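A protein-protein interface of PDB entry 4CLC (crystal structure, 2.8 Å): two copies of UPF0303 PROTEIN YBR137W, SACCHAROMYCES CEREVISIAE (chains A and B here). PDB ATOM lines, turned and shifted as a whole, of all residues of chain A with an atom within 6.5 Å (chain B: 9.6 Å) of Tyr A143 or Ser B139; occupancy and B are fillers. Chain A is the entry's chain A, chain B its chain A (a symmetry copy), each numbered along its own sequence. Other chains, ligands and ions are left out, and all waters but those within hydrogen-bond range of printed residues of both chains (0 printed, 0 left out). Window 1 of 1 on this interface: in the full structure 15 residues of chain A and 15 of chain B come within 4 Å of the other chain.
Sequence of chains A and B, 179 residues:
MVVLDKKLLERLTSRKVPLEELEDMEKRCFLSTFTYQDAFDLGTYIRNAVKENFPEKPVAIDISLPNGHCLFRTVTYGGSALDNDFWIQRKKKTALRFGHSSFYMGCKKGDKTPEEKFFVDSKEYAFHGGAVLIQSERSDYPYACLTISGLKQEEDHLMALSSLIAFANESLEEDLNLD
Leu A65 touches Tyr B141, and with the chains exchanged Tyr A141 touches Leu B65. Pro A66 touches its own counterpart, Pro B66. Positions printed for both chains: 30, 31, 32, 65, 66, 134, 135, 136, 137, 141, 142, 143 and 144. Of the 13 pairs that touch across the chains among the printed residues, 3 have their exchanged pair printed and touching as well.
The backbone carbonyl oxygen (O) of Ser A32 sits at hydrogen-bond distance from the side-chain hydroxyl (OH) of Tyr A143. The backbone NH (N) of Tyr A143 sits at hydrogen-bond distance from the backbone carbonyl oxygen (O) of Ile A134. N of Tyr B141 sits close to OG of Ser B139 (3.5 Å).
The backbone NH (N) of Phe A34 lies within hydrogen-bond range of the backbone carbonyl oxygen (O) of Arg B138 (3.3 Å). The backbone carbonyl oxygen (O) of Phe A34 lies within hydrogen-bond range of the side-chain hydroxyl (OG) of Ser B139 (3.0 Å). O of Phe A34 lies within hydrogen-bond range of N of Asp B140 (3.2 Å). OG1 of Thr A35 lies within hydrogen-bond range of OD2 of Asp B140 (2.6 Å).
Of chain B, only Arg B138 and Ser B139 come within 4 Å of Tyr A143. Printed residues of chain B within 4 Å of Phe A34: Arg B138, Ser B139, Asp B140 and Tyr B141. No residue of chain B comes within 4 Å of Pro A142. No residue of chain B comes within 4 Å of Ala A144. Of the printed residues of chain B, Ser A32 touches Arg B138. Printed residues of chain B within 4 Å of Pro A66: Pro B66 (3.6 Å) and Asn B67 (3.4 Å). Of the printed residues of chain B, Leu A65 touches Tyr B141 (3.7 Å). Of the printed residues of chain B, Tyr A141 touches Leu B65. The nearest residue of chain B that does not touch Tyr A143 is Ser B136 (4.9 Å). The nearest residue of chain A that does not touch Ser B139 is Thr A35 (5.2 Å). The nearest printed residue of chain A that does not touch Tyr B141 is Thr A35 (4.2 Å).
Printed residues of chain A that touch a printed residue of chain B: Ser A32, Thr A33, Phe A34, Thr A35, Leu A65, Pro A66, Tyr A141 and Tyr A143. Hydrophobic or aromatic side chains of chain A that line the printed part of chain B: Phe A34, Leu A65, Pro A66, Tyr A141 and Tyr A143. Hydrophobic or aromatic side chains of chain B that line the printed part of chain A: Leu B65, Pro B66 and Tyr B141. Among the printed residues, 13 pairs touch across the chains.
Among the printed residues, merely in contact across the chains: Ser A32 with Arg B138 (3.6 Å), Thr A33 with Arg B138 (3.4 Å), Phe A34 with Tyr B141 (3.97 Å), Leu A65 with Tyr B141 (3.7 Å), Pro A66 with Pro B66 (3.6 Å), Pro A66 with Asn B67 (3.4 Å), Tyr A141 with Leu B65 (3.7 Å), Tyr A143 with Arg B138 (3.9 Å) and Tyr A143 with Ser B139 (3.5 Å).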
ATOM      1  N   PHE A  30     -19.009  -9.423  -1.569  1.00  0.00           N
ATOM      2  CA  PHE A  30     -18.212 -10.555  -1.110  1.00  0.00           C
ATOM      3  C   PHE A  30     -18.804 -11.896  -1.530  1.00  0.00           C
ATOM      4  O   PHE A  30     -19.900 -11.964  -2.082  1.00  0.00           O
ATOM      5  CB  PHE A  30     -18.074 -10.523   0.407  1.00  0.00           C
ATOM      6  CG  PHE A  30     -19.291 -11.015   1.132  1.00  0.00           C
ATOM      7  CD1 PHE A  30     -20.387 -10.183   1.313  1.00  0.00           C
ATOM      8  CD2 PHE A  30     -19.339 -12.312   1.638  1.00  0.00           C
ATOM      9  CE1 PHE A  30     -21.511 -10.633   1.981  1.00  0.00           C
ATOM     10  CE2 PHE A  30     -20.462 -12.771   2.311  1.00  0.00           C
ATOM     11  CZ  PHE A  30     -21.549 -11.929   2.481  1.00  0.00           C
ATOM     12  N   LEU A  31     -18.087 -12.973  -1.241  1.00  0.00           N
ATOM     13  CA  LEU A  31     -18.522 -14.298  -1.653  1.00  0.00           C
ATOM     14  C   LEU A  31     -18.214 -15.341  -0.595  1.00  0.00           C
ATOM     15  O   LEU A  31     -17.342 -15.153   0.260  1.00  0.00           O
ATOM     16  CB  LEU A  31     -17.865 -14.709  -2.973  1.00  0.00           C
ATOM     17  CG  LEU A  31     -18.515 -14.276  -4.288  1.00  0.00           C
ATOM     18  CD1 LEU A  31     -18.271 -12.810  -4.606  1.00  0.00           C
ATOM     19  CD2 LEU A  31     -18.018 -15.163  -5.424  1.00  0.00           C
ATOM     20  N   SER A  32     -18.939 -16.448  -0.676  1.00  0.00           N
ATOM     21  CA  SER A  32     -18.724 -17.592   0.191  1.00  0.00           C
ATOM     22  C   SER A  32     -17.713 -18.511  -0.482  1.00  0.00           C
ATOM     23  O   SER A  32     -16.657 -18.810   0.073  1.00  0.00           O
ATOM     24  CB  SER A  32     -20.041 -18.314   0.471  1.00  0.00           C
ATOM     25  OG  SER A  32     -20.859 -18.326  -0.689  1.00  0.00           O
ATOM     26  N   THR A  33     -18.069 -18.993  -1.666  1.00  0.00           N
ATOM     27  CA  THR A  33     -17.111 -19.691  -2.515  1.00  0.00           C
ATOM     28  C   THR A  33     -16.418 -18.713  -3.460  1.00  0.00           C
ATOM     29  O   THR A  33     -17.037 -17.778  -3.969  1.00  0.00           O
ATOM     30  CB  THR A  33     -17.774 -20.802  -3.363  1.00  0.00           C
ATOM     31  OG1 THR A  33     -18.931 -20.276  -4.032  1.00  0.00           O
ATOM     32  CG2 THR A  33     -18.179 -21.980  -2.489  1.00  0.00           C
ATOM     33  N   PHE A  34     -15.118 -18.906  -3.645  1.00  0.00           N
ATOM     34  CA  PHE A  34     -14.414 -18.340  -4.784  1.00  0.00           C
ATOM     35  C   PHE A  34     -13.519 -19.424  -5.356  1.00  0.00           C
ATOM     36  O   PHE A  34     -12.521 -19.792  -4.743  1.00  0.00           O
ATOM     37  CB  PHE A  34     -13.601 -17.119  -4.357  1.00  0.00           C
ATOM     38  CG  PHE A  34     -12.940 -16.395  -5.492  1.00  0.00           C
ATOM     39  CD1 PHE A  34     -13.624 -15.409  -6.197  1.00  0.00           C
ATOM     40  CD2 PHE A  34     -11.634 -16.680  -5.841  1.00  0.00           C
ATOM     41  CE1 PHE A  34     -13.020 -14.725  -7.240  1.00  0.00           C
ATOM     42  CE2 PHE A  34     -11.018 -16.002  -6.875  1.00  0.00           C
ATOM     43  CZ  PHE A  34     -11.713 -15.021  -7.578  1.00  0.00           C
ATOM     44  N   THR A  35     -13.855 -19.908  -6.546  1.00  0.00           N
ATOM     45  CA  THR A  35     -13.103 -20.985  -7.186  1.00  0.00           C
ATOM     46  C   THR A  35     -12.791 -20.632  -8.626  1.00  0.00           C
ATOM     47  O   THR A  35     -13.233 -19.594  -9.121  1.00  0.00           O
ATOM     48  CB  THR A  35     -13.869 -22.319  -7.176  1.00  0.00           C
ATOM     49  OG1 THR A  35     -13.008 -23.360  -7.650  1.00  0.00           O
ATOM     50  CG2 THR A  35     -15.082 -22.253  -8.091  1.00  0.00           C
ATOM     51  N   SER A  64      -8.438 -10.946 -11.321  1.00  0.00           N
ATOM     52  CA  SER A  64      -7.076 -11.340 -10.973  1.00  0.00           C
ATOM     53  C   SER A  64      -6.948 -11.560  -9.473  1.00  0.00           C
ATOM     54  O   SER A  64      -7.670 -10.931  -8.701  1.00  0.00           O
ATOM     55  CB  SER A  64      -6.071 -10.269 -11.415  1.00  0.00           C
ATOM     56  OG  SER A  64      -5.777 -10.337 -12.799  1.00  0.00           O
ATOM     57  N   LEU A  65      -6.026 -12.437  -9.068  1.00  0.00           N
ATOM     58  CA  LEU A  65      -5.689 -12.624  -7.652  1.00  0.00           C
ATOM     59  C   LEU A  65      -4.734 -11.526  -7.198  1.00  0.00           C
ATOM     60  O   LEU A  65      -4.085 -10.896  -8.036  1.00  0.00           O
ATOM     61  CB  LEU A  65      -5.057 -13.994  -7.412  1.00  0.00           C
ATOM     62  CG  LEU A  65      -5.835 -15.242  -7.829  1.00  0.00           C
ATOM     63  CD1 LEU A  65      -5.022 -16.481  -7.481  1.00  0.00           C
ATOM     64  CD2 LEU A  65      -7.221 -15.289  -7.192  1.00  0.00           C
ATOM     65  N   PRO A  66      -4.638 -11.283  -5.876  1.00  0.00           N
ATOM     66  CA  PRO A  66      -3.748 -10.218  -5.383  1.00  0.00           C
ATOM     67  C   PRO A  66      -2.266 -10.399  -5.735  1.00  0.00           C
ATOM     68  O   PRO A  66      -1.520  -9.430  -5.618  1.00  0.00           O
ATOM     69  CB  PRO A  66      -3.941 -10.266  -3.852  1.00  0.00           C
ATOM     70  CG  PRO A  66      -4.700 -11.530  -3.569  1.00  0.00           C
ATOM     71  CD  PRO A  66      -5.490 -11.820  -4.801  1.00  0.00           C
ATOM     72  N   LEU A 133     -12.457  -4.555  -5.210  1.00  0.00           N
ATOM     73  CA  LEU A 133     -11.967  -5.772  -4.574  1.00  0.00           C
ATOM     74  C   LEU A 133     -13.102  -6.738  -4.318  1.00  0.00           C
ATOM     75  O   LEU A 133     -14.117  -6.362  -3.712  1.00  0.00           O
ATOM     76  CB  LEU A 133     -11.261  -5.457  -3.257  1.00  0.00           C
ATOM     77  CG  LEU A 133      -9.989  -4.629  -3.322  1.00  0.00           C
ATOM     78  CD1 LEU A 133      -9.610  -4.113  -1.952  1.00  0.00           C
ATOM     79  CD2 LEU A 133      -8.886  -5.473  -3.897  1.00  0.00           C
ATOM     80  N   ILE A 134     -12.938  -7.971  -4.791  1.00  0.00           N
ATOM     81  CA  ILE A 134     -13.839  -9.051  -4.417  1.00  0.00           C
ATOM     82  C   ILE A 134     -13.460  -9.468  -3.021  1.00  0.00           C
ATOM     83  O   ILE A 134     -12.290  -9.693  -2.745  1.00  0.00           O
ATOM     84  CB  ILE A 134     -13.736 -10.285  -5.333  1.00  0.00           C
ATOM     85  CG1 ILE A 134     -14.034  -9.947  -6.787  1.00  0.00           C
ATOM     86  CG2 ILE A 134     -14.688 -11.355  -4.873  1.00  0.00           C
ATOM     87  CD1 ILE A 134     -13.911 -11.159  -7.664  1.00  0.00           C
ATOM     88  N   GLN A 135     -14.441  -9.622  -2.146  1.00  0.00           N
ATOM     89  CA  GLN A 135     -14.138  -9.812  -0.739  1.00  0.00           C
ATOM     90  C   GLN A 135     -14.529 -11.194  -0.253  1.00  0.00           C
ATOM     91  O   GLN A 135     -15.315 -11.906  -0.883  1.00  0.00           O
ATOM     92  CB  GLN A 135     -14.834  -8.755   0.112  1.00  0.00           C
ATOM     93  CG  GLN A 135     -13.906  -8.049   1.082  1.00  0.00           C
ATOM     94  CD  GLN A 135     -13.170  -6.887   0.445  1.00  0.00           C
ATOM     95  OE1 GLN A 135     -13.690  -6.230  -0.464  1.00  0.00           O
ATOM     96  NE2 GLN A 135     -11.958  -6.614   0.928  1.00  0.00           N
ATOM     97  N   SER A 136     -13.930 -11.591   0.859  1.00  0.00           N
ATOM     98  CA  SER A 136     -14.280 -12.855   1.457  1.00  0.00           C
ATOM     99  C   SER A 136     -15.041 -12.583   2.762  1.00  0.00           C
ATOM    100  O   SER A 136     -14.704 -11.656   3.523  1.00  0.00           O
ATOM    101  CB  SER A 136     -13.014 -13.700   1.683  1.00  0.00           C
ATOM    102  OG  SER A 136     -13.247 -14.850   2.480  1.00  0.00           O
ATOM    103  N   GLU A 137     -16.108 -13.354   2.977  1.00  0.00           N
ATOM    104  CA  GLU A 137     -16.627 -13.566   4.321  1.00  0.00           C
ATOM    105  C   GLU A 137     -15.589 -14.440   5.005  1.00  0.00           C
ATOM    106  O   GLU A 137     -14.799 -15.080   4.308  1.00  0.00           O
ATOM    107  CB  GLU A 137     -17.991 -14.238   4.295  1.00  0.00           C
ATOM    108  N   TYR A 141      -9.225 -10.072   4.502  1.00  0.00           N
ATOM    109  CA  TYR A 141      -8.462  -9.674   3.324  1.00  0.00           C
ATOM    110  C   TYR A 141      -9.052 -10.265   2.038  1.00  0.00           C
ATOM    111  O   TYR A 141      -9.493 -11.419   2.025  1.00  0.00           O
ATOM    112  CB  TYR A 141      -6.988 -10.076   3.517  1.00  0.00           C
ATOM    113  CG  TYR A 141      -6.452  -9.565   4.835  1.00  0.00           C
ATOM    114  CD1 TYR A 141      -6.286  -8.203   5.049  1.00  0.00           C
ATOM    115  CD2 TYR A 141      -6.160 -10.436   5.886  1.00  0.00           C
ATOM    116  CE1 TYR A 141      -5.823  -7.721   6.267  1.00  0.00           C
ATOM    117  CE2 TYR A 141      -5.693  -9.960   7.113  1.00  0.00           C
ATOM    118  CZ  TYR A 141      -5.527  -8.601   7.294  1.00  0.00           C
ATOM    119  OH  TYR A 141      -5.074  -8.101   8.495  1.00  0.00           O
ATOM    120  N   PRO A 142      -9.060  -9.463   0.956  1.00  0.00           N
ATOM    121  CA  PRO A 142      -9.704  -9.761  -0.331  1.00  0.00           C
ATOM    122  C   PRO A 142      -9.285 -11.072  -0.966  1.00  0.00           C
ATOM    123  O   PRO A 142      -8.108 -11.451  -0.909  1.00  0.00           O
ATOM    124  CB  PRO A 142      -9.269  -8.595  -1.224  1.00  0.00           C
ATOM    125  CG  PRO A 142      -8.187  -7.872  -0.469  1.00  0.00           C
ATOM    126  CD  PRO A 142      -8.482  -8.110   0.968  1.00  0.00           C
ATOM    127  N   TYR A 143     -10.274 -11.745  -1.549  1.00  0.00           N
ATOM    128  CA  TYR A 143     -10.094 -12.901  -2.425  1.00  0.00           C
ATOM    129  C   TYR A 143      -9.228 -12.569  -3.637  1.00  0.00           C
ATOM    130  O   TYR A 143      -8.245 -13.248  -3.947  1.00  0.00           O
ATOM    131  CB  TYR A 143     -11.456 -13.393  -2.944  1.00  0.00           C
ATOM    132  CG  TYR A 143     -12.191 -14.443  -2.127  1.00  0.00           C
ATOM    133  CD1 TYR A 143     -11.563 -15.624  -1.738  1.00  0.00           C
ATOM    134  CD2 TYR A 143     -13.531 -14.264  -1.783  1.00  0.00           C
ATOM    135  CE1 TYR A 143     -12.242 -16.582  -1.011  1.00  0.00           C
ATOM    136  CE2 TYR A 143     -14.215 -15.213  -1.065  1.00  0.00           C
ATOM    137  CZ  TYR A 143     -13.566 -16.371  -0.678  1.00  0.00           C
ATOM    138  OH  TYR A 143     -14.247 -17.326   0.041  1.00  0.00           O
ATOM    139  N   ALA A 144      -9.650 -11.523  -4.338  1.00  0.00           N
ATOM    140  CA  ALA A 144      -9.124 -11.174  -5.640  1.00  0.00           C
ATOM    141  C   ALA A 144      -9.629  -9.800  -6.021  1.00  0.00           C
ATOM    142  O   ALA A 144     -10.429  -9.206  -5.303  1.00  0.00           O
ATOM    143  CB  ALA A 144      -9.548 -12.195  -6.671  1.00  0.00           C
ATOM    144  N   CYS A 145      -9.190  -9.307  -7.168  1.00  0.00           N
ATOM    145  CA  CYS A 145      -9.651  -8.008  -7.636  1.00  0.00           C
ATOM    146  C   CYS A 145     -10.441  -8.166  -8.922  1.00  0.00           C
ATOM    147  O   CYS A 145     -10.135  -9.041  -9.741  1.00  0.00           O
ATOM    148  CB  CYS A 145      -8.473  -7.058  -7.850  1.00  0.00           C
ATOM    149  SG  CYS A 145      -8.920  -5.376  -8.317  1.00  0.00           S
ATOM    150  N   LYS B  27      -1.673 -29.544   1.154  1.00  0.00           N
ATOM    151  CA  LYS B  27      -3.101 -29.281   0.945  1.00  0.00           C
ATOM    152  C   LYS B  27      -3.867 -29.352   2.270  1.00  0.00           C
ATOM    153  O   LYS B  27      -4.940 -28.753   2.418  1.00  0.00           O
ATOM    154  CB  LYS B  27      -3.700 -30.267  -0.085  1.00  0.00           C
ATOM    155  N   CYS B  29      -2.969 -28.049   5.084  1.00  0.00           N
ATOM    156  CA  CYS B  29      -2.831 -26.859   5.922  1.00  0.00           C
ATOM    157  C   CYS B  29      -3.783 -25.786   5.438  1.00  0.00           C
ATOM    158  O   CYS B  29      -3.517 -25.148   4.421  1.00  0.00           O
ATOM    159  CB  CYS B  29      -1.401 -26.302   5.876  1.00  0.00           C
ATOM    160  SG  CYS B  29      -0.073 -27.502   5.600  1.00  0.00           S
ATOM    161  N   PHE B  30      -4.851 -25.545   6.200  1.00  0.00           N
ATOM    162  CA  PHE B  30      -5.821 -24.515   5.842  1.00  0.00           C
ATOM    163  C   PHE B  30      -6.576 -23.977   7.052  1.00  0.00           C
ATOM    164  O   PHE B  30      -6.437 -24.480   8.165  1.00  0.00           O
ATOM    165  CB  PHE B  30      -6.821 -25.061   4.831  1.00  0.00           C
ATOM    166  CG  PHE B  30      -7.882 -25.926   5.441  1.00  0.00           C
ATOM    167  CD1 PHE B  30      -7.617 -27.253   5.747  1.00  0.00           C
ATOM    168  CD2 PHE B  30      -9.150 -25.413   5.706  1.00  0.00           C
ATOM    169  CE1 PHE B  30      -8.594 -28.055   6.310  1.00  0.00           C
ATOM    170  CE2 PHE B  30     -10.135 -26.211   6.269  1.00  0.00           C
ATOM    171  CZ  PHE B  30      -9.855 -27.533   6.572  1.00  0.00           C
ATOM    172  N   LEU B  31      -7.405 -22.966   6.828  1.00  0.00           N
ATOM    173  CA  LEU B  31      -8.127 -22.330   7.918  1.00  0.00           C
ATOM    174  C   LEU B  31      -9.533 -21.942   7.504  1.00  0.00           C
ATOM    175  O   LEU B  31      -9.837 -21.792   6.316  1.00  0.00           O
ATOM    176  CB  LEU B  31      -7.386 -21.088   8.420  1.00  0.00           C
ATOM    177  CG  LEU B  31      -6.290 -21.255   9.472  1.00  0.00           C
ATOM    178  CD1 LEU B  31      -4.999 -21.806   8.891  1.00  0.00           C
ATOM    179  CD2 LEU B  31      -6.041 -19.923  10.171  1.00  0.00           C
ATOM    180  N   SER B  32     -10.383 -21.774   8.508  1.00  0.00           N
ATOM    181  CA  SER B  32     -11.745 -21.313   8.313  1.00  0.00           C
ATOM    182  C   SER B  32     -11.746 -19.793   8.395  1.00  0.00           C
ATOM    183  O   SER B  32     -12.151 -19.105   7.459  1.00  0.00           O
ATOM    184  CB  SER B  32     -12.679 -21.932   9.354  1.00  0.00           C
ATOM    185  OG  SER B  32     -12.033 -22.022  10.614  1.00  0.00           O
ATOM    186  N   LEU B  65       0.515 -11.599   2.943  1.00  0.00           N
ATOM    187  CA  LEU B  65      -0.534 -11.837   1.944  1.00  0.00           C
ATOM    188  C   LEU B  65       0.093 -11.992   0.563  1.00  0.00           C
ATOM    189  O   LEU B  65       1.228 -11.559   0.355  1.00  0.00           O
ATOM    190  CB  LEU B  65      -1.548 -10.694   1.929  1.00  0.00           C
ATOM    191  CG  LEU B  65      -2.274 -10.341   3.227  1.00  0.00           C
ATOM    192  CD1 LEU B  65      -3.239  -9.193   2.968  1.00  0.00           C
ATOM    193  CD2 LEU B  65      -2.992 -11.549   3.824  1.00  0.00           C
ATOM    194  N   PRO B  66      -0.632 -12.610  -0.390  1.00  0.00           N
ATOM    195  CA  PRO B  66      -0.067 -12.808  -1.736  1.00  0.00           C
ATOM    196  C   PRO B  66       0.311 -11.518  -2.475  1.00  0.00           C
ATOM    197  O   PRO B  66       1.043 -11.608  -3.458  1.00  0.00           O
ATOM    198  CB  PRO B  66      -1.192 -13.545  -2.494  1.00  0.00           C
ATOM    199  CG  PRO B  66      -2.408 -13.458  -1.619  1.00  0.00           C
ATOM    200  CD  PRO B  66      -1.902 -13.338  -0.221  1.00  0.00           C
ATOM    201  N   ASN B  67      -0.177 -10.358  -2.035  1.00  0.00           N
ATOM    202  CA  ASN B  67       0.216  -9.090  -2.646  1.00  0.00           C
ATOM    203  C   ASN B  67       1.449  -8.482  -1.967  1.00  0.00           C
ATOM    204  O   ASN B  67       1.859  -7.360  -2.280  1.00  0.00           O
ATOM    205  CB  ASN B  67      -0.938  -8.094  -2.598  1.00  0.00           C
ATOM    206  CG  ASN B  67      -1.257  -7.655  -1.186  1.00  0.00           C
ATOM    207  OD1 ASN B  67      -1.064  -8.412  -0.231  1.00  0.00           O
ATOM    208  ND2 ASN B  67      -1.734  -6.422  -1.040  1.00  0.00           N
ATOM    209  N   ILE B 134      -0.531 -20.806   3.330  1.00  0.00           N
ATOM    210  CA  ILE B 134      -1.707 -20.963   4.175  1.00  0.00           C
ATOM    211  C   ILE B 134      -2.895 -21.028   3.252  1.00  0.00           C
ATOM    212  O   ILE B 134      -3.036 -20.191   2.374  1.00  0.00           O
ATOM    213  CB  ILE B 134      -1.922 -19.796   5.156  1.00  0.00           C
ATOM    214  CG1 ILE B 134      -0.734 -19.604   6.088  1.00  0.00           C
ATOM    215  CG2 ILE B 134      -3.158 -20.030   5.979  1.00  0.00           C
ATOM    216  CD1 ILE B 134      -0.956 -18.451   7.023  1.00  0.00           C
ATOM    217  N   GLN B 135      -3.781 -21.987   3.472  1.00  0.00           N
ATOM    218  CA  GLN B 135      -4.832 -22.242   2.504  1.00  0.00           C
ATOM    219  C   GLN B 135      -6.206 -21.913   3.052  1.00  0.00           C
ATOM    220  O   GLN B 135      -6.410 -21.791   4.263  1.00  0.00           O
ATOM    221  CB  GLN B 135      -4.801 -23.695   2.042  1.00  0.00           C
ATOM    222  CG  GLN B 135      -4.811 -23.855   0.534  1.00  0.00           C
ATOM    223  CD  GLN B 135      -3.425 -23.754  -0.072  1.00  0.00           C
ATOM    224  OE1 GLN B 135      -2.430 -24.126   0.558  1.00  0.00           O
ATOM    225  NE2 GLN B 135      -3.352 -23.260  -1.309  1.00  0.00           N
ATOM    226  N   SER B 136      -7.146 -21.718   2.140  1.00  0.00           N
ATOM    227  CA  SER B 136      -8.508 -21.473   2.546  1.00  0.00           C
ATOM    228  C   SER B 136      -9.353 -22.702   2.181  1.00  0.00           C
ATOM    229  O   SER B 136      -9.168 -23.318   1.115  1.00  0.00           O
ATOM    230  CB  SER B 136      -9.031 -20.186   1.884  1.00  0.00           C
ATOM    231  OG  SER B 136     -10.429 -20.009   2.044  1.00  0.00           O
ATOM    232  N   GLU B 137     -10.230 -23.091   3.107  1.00  0.00           N
ATOM    233  CA  GLU B 137     -11.399 -23.884   2.752  1.00  0.00           C
ATOM    234  C   GLU B 137     -12.300 -22.927   1.988  1.00  0.00           C
ATOM    235  O   GLU B 137     -12.128 -21.714   2.121  1.00  0.00           O
ATOM    236  CB  GLU B 137     -12.096 -24.439   3.985  1.00  0.00           C
ATOM    237  N   ARG B 138     -13.221 -23.442   1.176  1.00  0.00           N
ATOM    238  CA  ARG B 138     -14.169 -22.579   0.460  1.00  0.00           C
ATOM    239  C   ARG B 138     -13.502 -21.775  -0.662  1.00  0.00           C
ATOM    240  O   ARG B 138     -14.143 -20.935  -1.299  1.00  0.00           O
ATOM    241  CB  ARG B 138     -14.917 -21.620   1.441  1.00  0.00           C
ATOM    242  N   SER B 139     -12.206 -21.973  -0.865  1.00  0.00           N
ATOM    243  CA  SER B 139     -11.543 -21.292  -1.968  1.00  0.00           C
ATOM    244  C   SER B 139     -10.433 -22.134  -2.607  1.00  0.00           C
ATOM    245  O   SER B 139      -9.791 -22.947  -1.938  1.00  0.00           O
ATOM    246  CB  SER B 139     -10.983 -19.952  -1.491  1.00  0.00           C
ATOM    247  OG  SER B 139     -10.538 -19.183  -2.593  1.00  0.00           O
ATOM    248  N   ASP B 140     -10.222 -21.927  -3.905  1.00  0.00           N
ATOM    249  CA  ASP B 140      -9.177 -22.629  -4.648  1.00  0.00           C
ATOM    250  C   ASP B 140      -7.795 -22.000  -4.473  1.00  0.00           C
ATOM    251  O   ASP B 140      -6.778 -22.585  -4.863  1.00  0.00           O
ATOM    252  CB  ASP B 140      -9.517 -22.668  -6.142  1.00  0.00           C
ATOM    253  CG  ASP B 140     -10.128 -23.994  -6.579  1.00  0.00           C
ATOM    254  OD1 ASP B 140     -10.248 -24.927  -5.752  1.00  0.00           O
ATOM    255  OD2 ASP B 140     -10.479 -24.108  -7.770  1.00  0.00           O
ATOM    256  N   TYR B 141      -7.760 -20.800  -3.901  1.00  0.00           N
ATOM    257  CA  TYR B 141      -6.532 -20.012  -3.890  1.00  0.00           C
ATOM    258  C   TYR B 141      -6.164 -19.552  -2.475  1.00  0.00           C
ATOM    259  O   TYR B 141      -7.042 -19.185  -1.688  1.00  0.00           O
ATOM    260  CB  TYR B 141      -6.685 -18.824  -4.857  1.00  0.00           C
ATOM    261  CG  TYR B 141      -7.142 -19.287  -6.222  1.00  0.00           C
ATOM    262  CD1 TYR B 141      -6.305 -20.051  -7.024  1.00  0.00           C
ATOM    263  CD2 TYR B 141      -8.426 -19.008  -6.691  1.00  0.00           C
ATOM    264  CE1 TYR B 141      -6.725 -20.507  -8.267  1.00  0.00           C
ATOM    265  CE2 TYR B 141      -8.856 -19.462  -7.939  1.00  0.00           C
ATOM    266  CZ  TYR B 141      -7.999 -20.211  -8.721  1.00  0.00           C
ATOM    267  OH  TYR B 141      -8.396 -20.676  -9.955  1.00  0.00           O
ATOM    268  N   PRO B 142      -4.855 -19.580  -2.155  1.00  0.00           N
ATOM    269  CA  PRO B 142      -4.292 -19.329  -0.821  1.00  0.00           C
ATOM    270  C   PRO B 142      -4.698 -18.011  -0.193  1.00  0.00           C
ATOM    271  O   PRO B 142      -4.794 -16.989  -0.883  1.00  0.00           O
ATOM    272  CB  PRO B 142      -2.779 -19.336  -1.068  1.00  0.00           C
ATOM    273  CG  PRO B 142      -2.601 -19.308  -2.563  1.00  0.00           C
ATOM    274  CD  PRO B 142      -3.812 -19.968  -3.117  1.00  0.00           C
ATOM    275  N   TYR B 143      -4.944 -18.073   1.114  1.00  0.00           N
ATOM    276  CA  TYR B 143      -5.117 -16.914   1.986  1.00  0.00           C
ATOM    277  C   TYR B 143      -3.895 -16.002   1.974  1.00  0.00           C
ATOM    278  O   TYR B 143      -3.982 -14.790   1.759  1.00  0.00           O
ATOM    279  CB  TYR B 143      -5.346 -17.370   3.437  1.00  0.00           C
ATOM    280  CG  TYR B 143      -6.776 -17.610   3.890  1.00  0.00           C
ATOM    281  CD1 TYR B 143      -7.762 -16.643   3.711  1.00  0.00           C
ATOM    282  CD2 TYR B 143      -7.126 -18.797   4.537  1.00  0.00           C
ATOM    283  CE1 TYR B 143      -9.056 -16.860   4.141  1.00  0.00           C
ATOM    284  CE2 TYR B 143      -8.409 -19.019   4.972  1.00  0.00           C
ATOM    285  CZ  TYR B 143      -9.374 -18.048   4.770  1.00  0.00           C
ATOM    286  OH  TYR B 143     -10.661 -18.265   5.204  1.00  0.00           O
ATOM    287  N   ALA B 144      -2.752 -16.618   2.252  1.00  0.00           N
ATOM    288  CA  ALA B 144      -1.515 -15.917   2.521  1.00  0.00           C
ATOM    289  C   ALA B 144      -0.378 -16.914   2.531  1.00  0.00           C
ATOM    290  O   ALA B 144      -0.598 -18.116   2.412  1.00  0.00           O
ATOM    291  CB  ALA B 144      -1.594 -15.196   3.847  1.00  0.00           C
